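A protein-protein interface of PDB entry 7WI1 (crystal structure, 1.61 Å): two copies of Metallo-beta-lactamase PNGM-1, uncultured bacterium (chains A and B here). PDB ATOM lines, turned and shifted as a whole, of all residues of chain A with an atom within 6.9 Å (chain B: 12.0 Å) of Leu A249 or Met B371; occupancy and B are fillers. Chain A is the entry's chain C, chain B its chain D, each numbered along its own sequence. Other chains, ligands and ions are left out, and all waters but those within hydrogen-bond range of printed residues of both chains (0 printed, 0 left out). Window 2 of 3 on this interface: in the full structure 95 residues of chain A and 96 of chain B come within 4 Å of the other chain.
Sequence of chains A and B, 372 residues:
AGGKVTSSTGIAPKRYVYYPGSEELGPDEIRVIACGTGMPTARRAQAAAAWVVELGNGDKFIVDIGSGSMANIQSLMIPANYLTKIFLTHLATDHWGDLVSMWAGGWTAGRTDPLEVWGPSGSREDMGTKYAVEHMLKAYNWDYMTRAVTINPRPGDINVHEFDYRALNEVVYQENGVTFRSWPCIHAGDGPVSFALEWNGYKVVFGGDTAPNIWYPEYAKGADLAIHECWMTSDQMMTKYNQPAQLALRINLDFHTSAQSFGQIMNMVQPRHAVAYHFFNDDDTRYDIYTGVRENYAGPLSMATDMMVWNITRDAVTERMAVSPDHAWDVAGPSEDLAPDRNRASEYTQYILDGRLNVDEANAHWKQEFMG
Of the 14 printed residues of chain B, 6 touch a printed residue of chain A. Hydrophobic or aromatic side chains of chain B that line the printed part of chain A: Trp B366, Phe B370 and Met B371. Of the 15 printed residues of chain A, 7 touch a printed residue of chain B. Hydrophobic or aromatic side chains of chain A that line the printed part of chain B: Met A238, Leu A249 and Leu A253. Among the printed residues, 12 pairs touch across the chains. Among the printed residues, no Asp or Glu carboxylate lies within 4 Å of a Lys or Arg side-chain nitrogen of the other chain.
No position is printed for both chains. Of the 12 pairs that touch across the chains among the printed residues, none has its exchanged pair printed and touching as well.
Among the printed residues, merely in contact across the chains: Ser A234 with Trp B366 (3.2 Å), Ala A245 with Phe B370 (3.5 Å), Leu A249 with Met B371 (3.6 Å), Leu A249 with Trp B366 (3.6 Å), Met A238 with Phe B370 (3.8 Å), Ser A234 with Phe B370 (3.8 Å), Asn A252 with Trp B366 (3.9 Å), Leu A249 with Phe B370 (3.9 Å), Leu A253 with Lys B367 (3.9 Å), Leu A253 with Trp B366 (3.98 Å) and Leu A253 with Asn B363 (3.99 Å).
O of Asp A254 sits at hydrogen-bond distance from NH1 of Arg B356 (2.7 Å).
OG of Ser A234 is in hydrogen-bond range of ND2 of Asn A252. OG of Ser A234 sits at hydrogen-bond distance from O of Ala A248 (2.6 Å). The side-chain amide oxygen (OD1) of Asn B363 lies within hydrogen-bond range of the indole nitrogen (NE1) of Trp B366 (2.8 Å). OD2 of Asp A254 is in salt-bridge range of NH1 of Arg A250 (2.9 Å). O of Val B359 is in hydrogen-bond range of ND2 of Asn B363, 2.8 Å away.
Printed residues of chain B within 4 Å of Leu A249: Trp B366, Phe B370 and Met B371. Of chain A, only Leu A249 comes within 4 Å of Met B371. Ser A234 touches just these residues of chain B: Trp B366 and Phe B370. Of chain B, only Phe B370 comes within 4 Å of Ala A245. Gln A246 touches none of the printed residues of chain B. No residue of chain B comes within 4 Å of Leu A247. No residue of chain B comes within 4 Å of Arg A250. Asn A252 touches just one residue of chain B: Trp B366 (3.9 Å). Of the printed residues of chain A, Asn B363 touches Leu A253. Of the printed residues of chain B, Asp A254 touches Arg B356. Asp B360 touches none of the printed residues of chain A. Gln A243 touches none of the printed residues of chain B. The nearest printed residue of chain B that does not touch Leu A253 is Arg B356 (4.7 Å).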
ATOM      1  N   SER A 234      -0.252   5.360   5.982  1.00  0.00           N
ATOM      2  CA  SER A 234      -1.345   4.469   6.408  1.00  0.00           C
ATOM      3  C   SER A 234      -2.691   5.142   6.121  1.00  0.00           C
ATOM      4  O   SER A 234      -3.613   4.430   5.675  1.00  0.00           O
ATOM      5  CB  SER A 234      -1.118   4.121   7.851  1.00  0.00           C
ATOM      6  OG  SER A 234       0.005   3.281   7.971  1.00  0.00           O
ATOM      7  N   MET A 237      -3.298   4.625   2.502  1.00  0.00           N
ATOM      8  CA  MET A 237      -3.662   3.205   2.282  1.00  0.00           C
ATOM      9  C   MET A 237      -5.169   3.046   2.521  1.00  0.00           C
ATOM     10  O   MET A 237      -5.824   2.373   1.732  1.00  0.00           O
ATOM     11  CB  MET A 237      -2.889   2.245   3.189  1.00  0.00           C
ATOM     12  CG  MET A 237      -1.362   2.201   2.947  1.00  0.00           C
ATOM     13  SD  MET A 237      -0.900   1.724   1.252  1.00  0.00           S
ATOM     14  CE  MET A 237      -1.609   0.082   1.114  1.00  0.00           C
ATOM     15  N   MET A 238      -5.709   3.706   3.542  1.00  0.00           N
ATOM     16  CA  MET A 238      -7.173   3.652   3.828  1.00  0.00           C
ATOM     17  C   MET A 238      -7.957   4.377   2.732  1.00  0.00           C
ATOM     18  O   MET A 238      -8.928   3.771   2.203  1.00  0.00           O
ATOM     19  CB  MET A 238      -7.449   4.243   5.211  1.00  0.00           C
ATOM     20  CG  MET A 238      -6.923   3.343   6.302  1.00  0.00           C
ATOM     21  SD  MET A 238      -7.350   4.024   7.933  1.00  0.00           S
ATOM     22  CE  MET A 238      -9.073   3.533   8.043  1.00  0.00           C
ATOM     23  N   GLN A 243      -8.449   0.068   3.008  1.00  0.00           N
ATOM     24  CA  GLN A 243      -7.830  -0.873   3.981  1.00  0.00           C
ATOM     25  C   GLN A 243      -8.464  -0.665   5.345  1.00  0.00           C
ATOM     26  O   GLN A 243      -8.703   0.484   5.710  1.00  0.00           O
ATOM     27  CB  GLN A 243      -6.347  -0.586   4.202  1.00  0.00           C
ATOM     28  CG  GLN A 243      -5.486  -0.587   2.956  1.00  0.00           C
ATOM     29  CD  GLN A 243      -5.193  -1.975   2.453  1.00  0.00           C
ATOM     30  OE1 GLN A 243      -6.059  -2.850   2.453  1.00  0.00           O
ATOM     31  NE2 GLN A 243      -3.960  -2.182   2.019  1.00  0.00           N
ATOM     32  N   PRO A 244      -8.658  -1.739   6.157  1.00  0.00           N
ATOM     33  CA  PRO A 244      -8.925  -1.584   7.591  1.00  0.00           C
ATOM     34  C   PRO A 244      -7.747  -0.908   8.311  1.00  0.00           C
ATOM     35  O   PRO A 244      -6.610  -1.192   7.965  1.00  0.00           O
ATOM     36  CB  PRO A 244      -9.113  -3.010   8.136  1.00  0.00           C
ATOM     37  CG  PRO A 244      -9.240  -3.906   6.906  1.00  0.00           C
ATOM     38  CD  PRO A 244      -8.631  -3.148   5.737  1.00  0.00           C
ATOM     39  N   ALA A 245      -8.035  -0.056   9.302  1.00  0.00           N
ATOM     40  CA  ALA A 245      -7.041   0.748  10.053  1.00  0.00           C
ATOM     41  C   ALA A 245      -5.858  -0.116  10.518  1.00  0.00           C
ATOM     42  O   ALA A 245      -4.714   0.371  10.413  1.00  0.00           O
ATOM     43  CB  ALA A 245      -7.694   1.446  11.228  1.00  0.00           C
ATOM     44  N   GLN A 246      -6.089  -1.320  11.059  1.00  0.00           N
ATOM     45  CA  GLN A 246      -4.994  -2.131  11.664  1.00  0.00           C
ATOM     46  C   GLN A 246      -4.095  -2.708  10.549  1.00  0.00           C
ATOM     47  O   GLN A 246      -2.885  -2.787  10.769  1.00  0.00           O
ATOM     48  CB  GLN A 246      -5.555  -3.177  12.643  1.00  0.00           C
ATOM     49  CG  GLN A 246      -5.921  -4.517  12.021  1.00  0.00           C
ATOM     50  CD  GLN A 246      -4.752  -5.472  11.923  1.00  0.00           C
ATOM     51  OE1 GLN A 246      -3.795  -5.414  12.700  1.00  0.00           O
ATOM     52  NE2 GLN A 246      -4.817  -6.367  10.946  1.00  0.00           N
ATOM     53  N   LEU A 247      -4.642  -3.078   9.391  1.00  0.00           N
ATOM     54  CA  LEU A 247      -3.828  -3.560   8.236  1.00  0.00           C
ATOM     55  C   LEU A 247      -3.008  -2.389   7.674  1.00  0.00           C
ATOM     56  O   LEU A 247      -1.799  -2.554   7.487  1.00  0.00           O
ATOM     57  CB  LEU A 247      -4.714  -4.159   7.143  1.00  0.00           C
ATOM     58  CG  LEU A 247      -3.951  -5.030   6.148  1.00  0.00           C
ATOM     59  CD1 LEU A 247      -3.834  -6.453   6.685  1.00  0.00           C
ATOM     60  CD2 LEU A 247      -4.613  -5.018   4.782  1.00  0.00           C
ATOM     61  N   ALA A 248      -3.641  -1.233   7.450  1.00  0.00           N
ATOM     62  CA  ALA A 248      -2.963  -0.009   6.961  1.00  0.00           C
ATOM     63  C   ALA A 248      -1.830   0.378   7.929  1.00  0.00           C
ATOM     64  O   ALA A 248      -0.785   0.875   7.478  1.00  0.00           O
ATOM     65  CB  ALA A 248      -3.964   1.103   6.762  1.00  0.00           C
ATOM     66  N   LEU A 249      -2.018   0.140   9.231  1.00  0.00           N
ATOM     67  CA  LEU A 249      -0.972   0.374  10.253  1.00  0.00           C
ATOM     68  C   LEU A 249       0.193  -0.599  10.025  1.00  0.00           C
ATOM     69  O   LEU A 249       1.346  -0.127  10.008  1.00  0.00           O
ATOM     70  CB  LEU A 249      -1.615   0.169  11.625  1.00  0.00           C
ATOM     71  CG  LEU A 249      -0.725   0.435  12.830  1.00  0.00           C
ATOM     72  CD1 LEU A 249      -0.383   1.908  12.939  1.00  0.00           C
ATOM     73  CD2 LEU A 249      -1.410  -0.045  14.106  1.00  0.00           C
ATOM     74  N   ARG A 250      -0.107  -1.890   9.820  1.00  0.00           N
ATOM     75  CA  ARG A 250       0.878  -3.000   9.638  1.00  0.00           C
ATOM     76  C   ARG A 250       1.720  -2.765   8.376  1.00  0.00           C
ATOM     77  O   ARG A 250       2.943  -2.964   8.422  1.00  0.00           O
ATOM     78  CB  ARG A 250       0.211  -4.378   9.498  1.00  0.00           C
ATOM     79  CG  ARG A 250      -0.400  -4.961  10.772  1.00  0.00           C
ATOM     80  CD  ARG A 250       0.591  -5.336  11.870  1.00  0.00           C
ATOM     81  NE  ARG A 250       0.806  -4.254  12.834  1.00  0.00           N
ATOM     82  CZ  ARG A 250       1.777  -4.200  13.750  1.00  0.00           C
ATOM     83  NH1 ARG A 250       2.672  -5.169  13.861  1.00  0.00           N
ATOM     84  NH2 ARG A 250       1.852  -3.153  14.556  1.00  0.00           N
ATOM     85  N   ILE A 251       1.079  -2.365   7.276  1.00  0.00           N
ATOM     86  CA  ILE A 251       1.777  -2.129   5.979  1.00  0.00           C
ATOM     87  C   ILE A 251       3.013  -1.254   6.224  1.00  0.00           C
ATOM     88  O   ILE A 251       4.085  -1.572   5.613  1.00  0.00           O
ATOM     89  CB  ILE A 251       0.817  -1.528   4.936  1.00  0.00           C
ATOM     90  CG1 ILE A 251      -0.045  -2.638   4.332  1.00  0.00           C
ATOM     91  CG2 ILE A 251       1.583  -0.731   3.876  1.00  0.00           C
ATOM     92  CD1 ILE A 251      -1.475  -2.247   4.118  1.00  0.00           C
ATOM     93  N   ASN A 252       2.894  -0.220   7.067  1.00  0.00           N
ATOM     94  CA  ASN A 252       3.978   0.766   7.295  1.00  0.00           C
ATOM     95  C   ASN A 252       4.883   0.367   8.461  1.00  0.00           C
ATOM     96  O   ASN A 252       5.868   1.076   8.699  1.00  0.00           O
ATOM     97  CB  ASN A 252       3.434   2.176   7.524  1.00  0.00           C
ATOM     98  CG  ASN A 252       3.341   2.937   6.225  1.00  0.00           C
ATOM     99  OD1 ASN A 252       4.364   3.193   5.617  1.00  0.00           O
ATOM    100  ND2 ASN A 252       2.145   3.220   5.766  1.00  0.00           N
ATOM    101  N   LEU A 253       4.584  -0.708   9.186  1.00  0.00           N
ATOM    102  CA  LEU A 253       5.429  -1.094  10.346  1.00  0.00           C
ATOM    103  C   LEU A 253       6.110  -2.428  10.053  1.00  0.00           C
ATOM    104  O   LEU A 253       7.321  -2.531  10.338  1.00  0.00           O
ATOM    105  CB  LEU A 253       4.583  -1.174  11.616  1.00  0.00           C
ATOM    106  CG  LEU A 253       4.435   0.091  12.482  1.00  0.00           C
ATOM    107  CD1 LEU A 253       5.382   1.217  12.110  1.00  0.00           C
ATOM    108  CD2 LEU A 253       3.003   0.587  12.466  1.00  0.00           C
ATOM    109  N   ASP A 254       5.393  -3.408   9.501  1.00  0.00           N
ATOM    110  CA  ASP A 254       5.965  -4.769   9.342  1.00  0.00           C
ATOM    111  C   ASP A 254       6.461  -4.990   7.909  1.00  0.00           C
ATOM    112  O   ASP A 254       7.556  -5.543   7.746  1.00  0.00           O
ATOM    113  CB  ASP A 254       4.962  -5.859   9.714  1.00  0.00           C
ATOM    114  CG  ASP A 254       4.553  -5.909  11.178  1.00  0.00           C
ATOM    115  OD1 ASP A 254       5.317  -5.426  12.049  1.00  0.00           O
ATOM    116  OD2 ASP A 254       3.460  -6.438  11.432  1.00  0.00           O
ATOM    117  N   ARG B 356      15.869  -7.097  11.479  1.00  0.00           N
ATOM    118  CA  ARG B 356      14.884  -5.983  11.603  1.00  0.00           C
ATOM    119  C   ARG B 356      15.481  -4.814  12.401  1.00  0.00           C
ATOM    120  O   ARG B 356      16.162  -5.082  13.421  1.00  0.00           O
ATOM    121  CB  ARG B 356      13.570  -6.453  12.223  1.00  0.00           C
ATOM    122  CG  ARG B 356      12.734  -7.333  11.303  1.00  0.00           C
ATOM    123  CD  ARG B 356      11.236  -7.243  11.539  1.00  0.00           C
ATOM    124  NE  ARG B 356      10.463  -8.154  10.691  1.00  0.00           N
ATOM    125  CZ  ARG B 356       9.719  -7.808   9.627  1.00  0.00           C
ATOM    126  NH1 ARG B 356       9.601  -6.537   9.252  1.00  0.00           N
ATOM    127  NH2 ARG B 356       9.059  -8.746   8.966  1.00  0.00           N
ATOM    128  N   VAL B 359      12.688   0.847  14.813  1.00  0.00           N
ATOM    129  CA  VAL B 359      12.269   2.188  14.306  1.00  0.00           C
ATOM    130  C   VAL B 359      11.114   2.701  15.181  1.00  0.00           C
ATOM    131  O   VAL B 359      10.363   3.530  14.715  1.00  0.00           O
ATOM    132  CB  VAL B 359      11.827   2.097  12.834  1.00  0.00           C
ATOM    133  CG1 VAL B 359      13.032   1.805  11.951  1.00  0.00           C
ATOM    134  CG2 VAL B 359      10.702   1.087  12.653  1.00  0.00           C
ATOM    135  N   ASP B 360      10.968   2.177  16.407  1.00  0.00           N
ATOM    136  CA  ASP B 360       9.828   2.563  17.292  1.00  0.00           C
ATOM    137  C   ASP B 360       9.757   4.081  17.525  1.00  0.00           C
ATOM    138  O   ASP B 360       8.662   4.641  17.379  1.00  0.00           O
ATOM    139  CB  ASP B 360       9.938   1.806  18.619  1.00  0.00           C
ATOM    140  CG  ASP B 360       9.721   0.321  18.468  1.00  0.00           C
ATOM    141  OD1 ASP B 360       9.171  -0.123  17.410  1.00  0.00           O
ATOM    142  OD2 ASP B 360      10.076  -0.398  19.417  1.00  0.00           O
ATOM    143  N   ALA B 362      11.060   6.611  15.869  1.00  0.00           N
ATOM    144  CA  ALA B 362      10.864   7.399  14.635  1.00  0.00           C
ATOM    145  C   ALA B 362       9.393   7.379  14.213  1.00  0.00           C
ATOM    146  O   ALA B 362       8.962   8.324  13.537  1.00  0.00           O
ATOM    147  CB  ALA B 362      11.754   6.808  13.563  1.00  0.00           C
ATOM    148  N   ASN B 363       8.647   6.330  14.567  1.00  0.00           N
ATOM    149  CA  ASN B 363       7.273   6.085  14.096  1.00  0.00           C
ATOM    150  C   ASN B 363       6.254   6.461  15.183  1.00  0.00           C
ATOM    151  O   ASN B 363       5.038   6.426  14.864  1.00  0.00           O
ATOM    152  CB  ASN B 363       7.109   4.649  13.610  1.00  0.00           C
ATOM    153  CG  ASN B 363       7.788   4.452  12.265  1.00  0.00           C
ATOM    154  OD1 ASN B 363       7.169   4.677  11.222  1.00  0.00           O
ATOM    155  ND2 ASN B 363       9.068   4.111  12.293  1.00  0.00           N
ATOM    156  N   ALA B 364       6.736   6.832  16.381  1.00  0.00           N
ATOM    157  CA  ALA B 364       5.884   6.961  17.598  1.00  0.00           C
ATOM    158  C   ALA B 364       4.877   8.099  17.396  1.00  0.00           C
ATOM    159  O   ALA B 364       3.687   7.901  17.668  1.00  0.00           O
ATOM    160  CB  ALA B 364       6.740   7.156  18.833  1.00  0.00           C
ATOM    161  N   HIS B 365       5.339   9.235  16.877  1.00  0.00           N
ATOM    162  CA  HIS B 365       4.504  10.447  16.673  1.00  0.00           C
ATOM    163  C   HIS B 365       3.349  10.117  15.711  1.00  0.00           C
ATOM    164  O   HIS B 365       2.179  10.266  16.132  1.00  0.00           O
ATOM    165  CB  HIS B 365       5.400  11.617  16.250  1.00  0.00           C
ATOM    166  CG  HIS B 365       4.876  12.974  16.583  1.00  0.00           C
ATOM    167  ND1 HIS B 365       3.868  13.581  15.847  1.00  0.00           N
ATOM    168  CD2 HIS B 365       5.250  13.868  17.527  1.00  0.00           C
ATOM    169  CE1 HIS B 365       3.628  14.784  16.338  1.00  0.00           C
ATOM    170  NE2 HIS B 365       4.461  14.982  17.372  1.00  0.00           N
ATOM    171  N   TRP B 366       3.604   9.629  14.483  1.00  0.00           N
ATOM    172  CA  TRP B 366       2.479   9.336  13.548  1.00  0.00           C
ATOM    173  C   TRP B 366       1.608   8.195  14.092  1.00  0.00           C
ATOM    174  O   TRP B 366       0.370   8.273  13.914  1.00  0.00           O
ATOM    175  CB  TRP B 366       2.932   9.073  12.092  1.00  0.00           C
ATOM    176  CG  TRP B 366       3.360   7.672  11.774  1.00  0.00           C
ATOM    177  CD1 TRP B 366       4.645   7.226  11.720  1.00  0.00           C
ATOM    178  CD2 TRP B 366       2.529   6.552  11.399  1.00  0.00           C
ATOM    179  NE1 TRP B 366       4.668   5.914  11.348  1.00  0.00           N
ATOM    180  CE2 TRP B 366       3.393   5.455  11.172  1.00  0.00           C
ATOM    181  CE3 TRP B 366       1.149   6.333  11.271  1.00  0.00           C
ATOM    182  CZ2 TRP B 366       2.934   4.198  10.805  1.00  0.00           C
ATOM    183  CZ3 TRP B 366       0.696   5.080  10.940  1.00  0.00           C
ATOM    184  CH2 TRP B 366       1.574   4.020  10.701  1.00  0.00           C
ATOM    185  N   LYS B 367       2.212   7.178  14.718  1.00  0.00           N
ATOM    186  CA  LYS B 367       1.540   5.926  15.192  1.00  0.00           C
ATOM    187  C   LYS B 367       0.479   6.249  16.264  1.00  0.00           C
ATOM    188  O   LYS B 367      -0.642   5.701  16.179  1.00  0.00           O
ATOM    189  CB  LYS B 367       2.594   4.985  15.782  1.00  0.00           C
ATOM    190  CG  LYS B 367       2.177   3.542  16.006  1.00  0.00           C
ATOM    191  CD  LYS B 367       3.357   2.590  15.842  1.00  0.00           C
ATOM    192  CE  LYS B 367       3.843   1.985  17.135  1.00  0.00           C
ATOM    193  NZ  LYS B 367       2.976   0.848  17.508  1.00  0.00           N
ATOM    194  N   GLN B 368       0.845   7.095  17.230  1.00  0.00           N
ATOM    195  CA  GLN B 368      -0.048   7.598  18.317  1.00  0.00           C
ATOM    196  C   GLN B 368      -1.214   8.396  17.698  1.00  0.00           C
ATOM    197  O   GLN B 368      -2.400   8.005  17.923  1.00  0.00           O
ATOM    198  CB  GLN B 368       0.797   8.430  19.279  1.00  0.00           C
ATOM    199  CG  GLN B 368       0.053   8.895  20.519  1.00  0.00           C
ATOM    200  CD  GLN B 368       0.894   9.884  21.287  1.00  0.00           C
ATOM    201  OE1 GLN B 368       0.774  11.093  21.117  1.00  0.00           O
ATOM    202  NE2 GLN B 368       1.783   9.371  22.120  1.00  0.00           N
ATOM    203  N   GLU B 369      -0.892   9.428  16.906  1.00  0.00           N
ATOM    204  CA  GLU B 369      -1.879  10.335  16.251  1.00  0.00           C
ATOM    205  C   GLU B 369      -2.815   9.509  15.349  1.00  0.00           C
ATOM    206  O   GLU B 369      -4.013   9.827  15.339  1.00  0.00           O
ATOM    207  CB  GLU B 369      -1.164  11.468  15.505  1.00  0.00           C
ATOM    208  CG  GLU B 369      -2.062  12.639  15.109  1.00  0.00           C
ATOM    209  CD  GLU B 369      -2.928  12.464  13.862  1.00  0.00           C
ATOM    210  OE1 GLU B 369      -2.793  11.431  13.162  1.00  0.00           O
ATOM    211  OE2 GLU B 369      -3.748  13.366  13.579  1.00  0.00           O
ATOM    212  N   PHE B 370      -2.317   8.475  14.643  1.00  0.00           N
ATOM    213  CA  PHE B 370      -3.112   7.631  13.703  1.00  0.00           C
ATOM    214  C   PHE B 370      -4.039   6.680  14.471  1.00  0.00           C
ATOM    215  O   PHE B 370      -5.187   6.472  14.023  1.00  0.00           O
ATOM    216  CB  PHE B 370      -2.223   6.802  12.768  1.00  0.00           C
ATOM    217  CG  PHE B 370      -2.971   5.849  11.861  1.00  0.00           C
ATOM    218  CD1 PHE B 370      -3.482   6.274  10.644  1.00  0.00           C
ATOM    219  CD2 PHE B 370      -3.173   4.529  12.223  1.00  0.00           C
ATOM    220  CE1 PHE B 370      -4.160   5.394   9.807  1.00  0.00           C
ATOM    221  CE2 PHE B 370      -3.850   3.653  11.392  1.00  0.00           C
ATOM    222  CZ  PHE B 370      -4.328   4.080  10.173  1.00  0.00           C
ATOM    223  N   MET B 371      -3.544   6.083  15.552  1.00  0.00           N
ATOM    224  CA  MET B 371      -4.318   5.137  16.403  1.00  0.00           C
ATOM    225  C   MET B 371      -5.521   5.861  17.055  1.00  0.00           C
ATOM    226  O   MET B 371      -6.590   5.236  17.121  1.00  0.00           O
ATOM    227  CB  MET B 371      -3.412   4.454  17.436  1.00  0.00           C
ATOM    228  CG  MET B 371      -2.791   3.153  16.898  1.00  0.00           C
ATOM    229  SD  MET B 371      -1.237   2.650  17.705  1.00  0.00           S
ATOM    230  CE  MET B 371      -1.356   0.865  17.606  1.00  0.00           C
ATOM    231  N   GLY B 372      -5.393   7.142  17.441  1.00  0.00           N
ATOM    232  CA  GLY B 372      -6.530   8.046  17.730  1.00  0.00           C
ATOM    233  C   GLY B 372      -7.001   8.789  16.482  1.00  0.00           C
ATOM    234  O   GLY B 372      -7.852   8.389  15.652  1.00  0.00           O
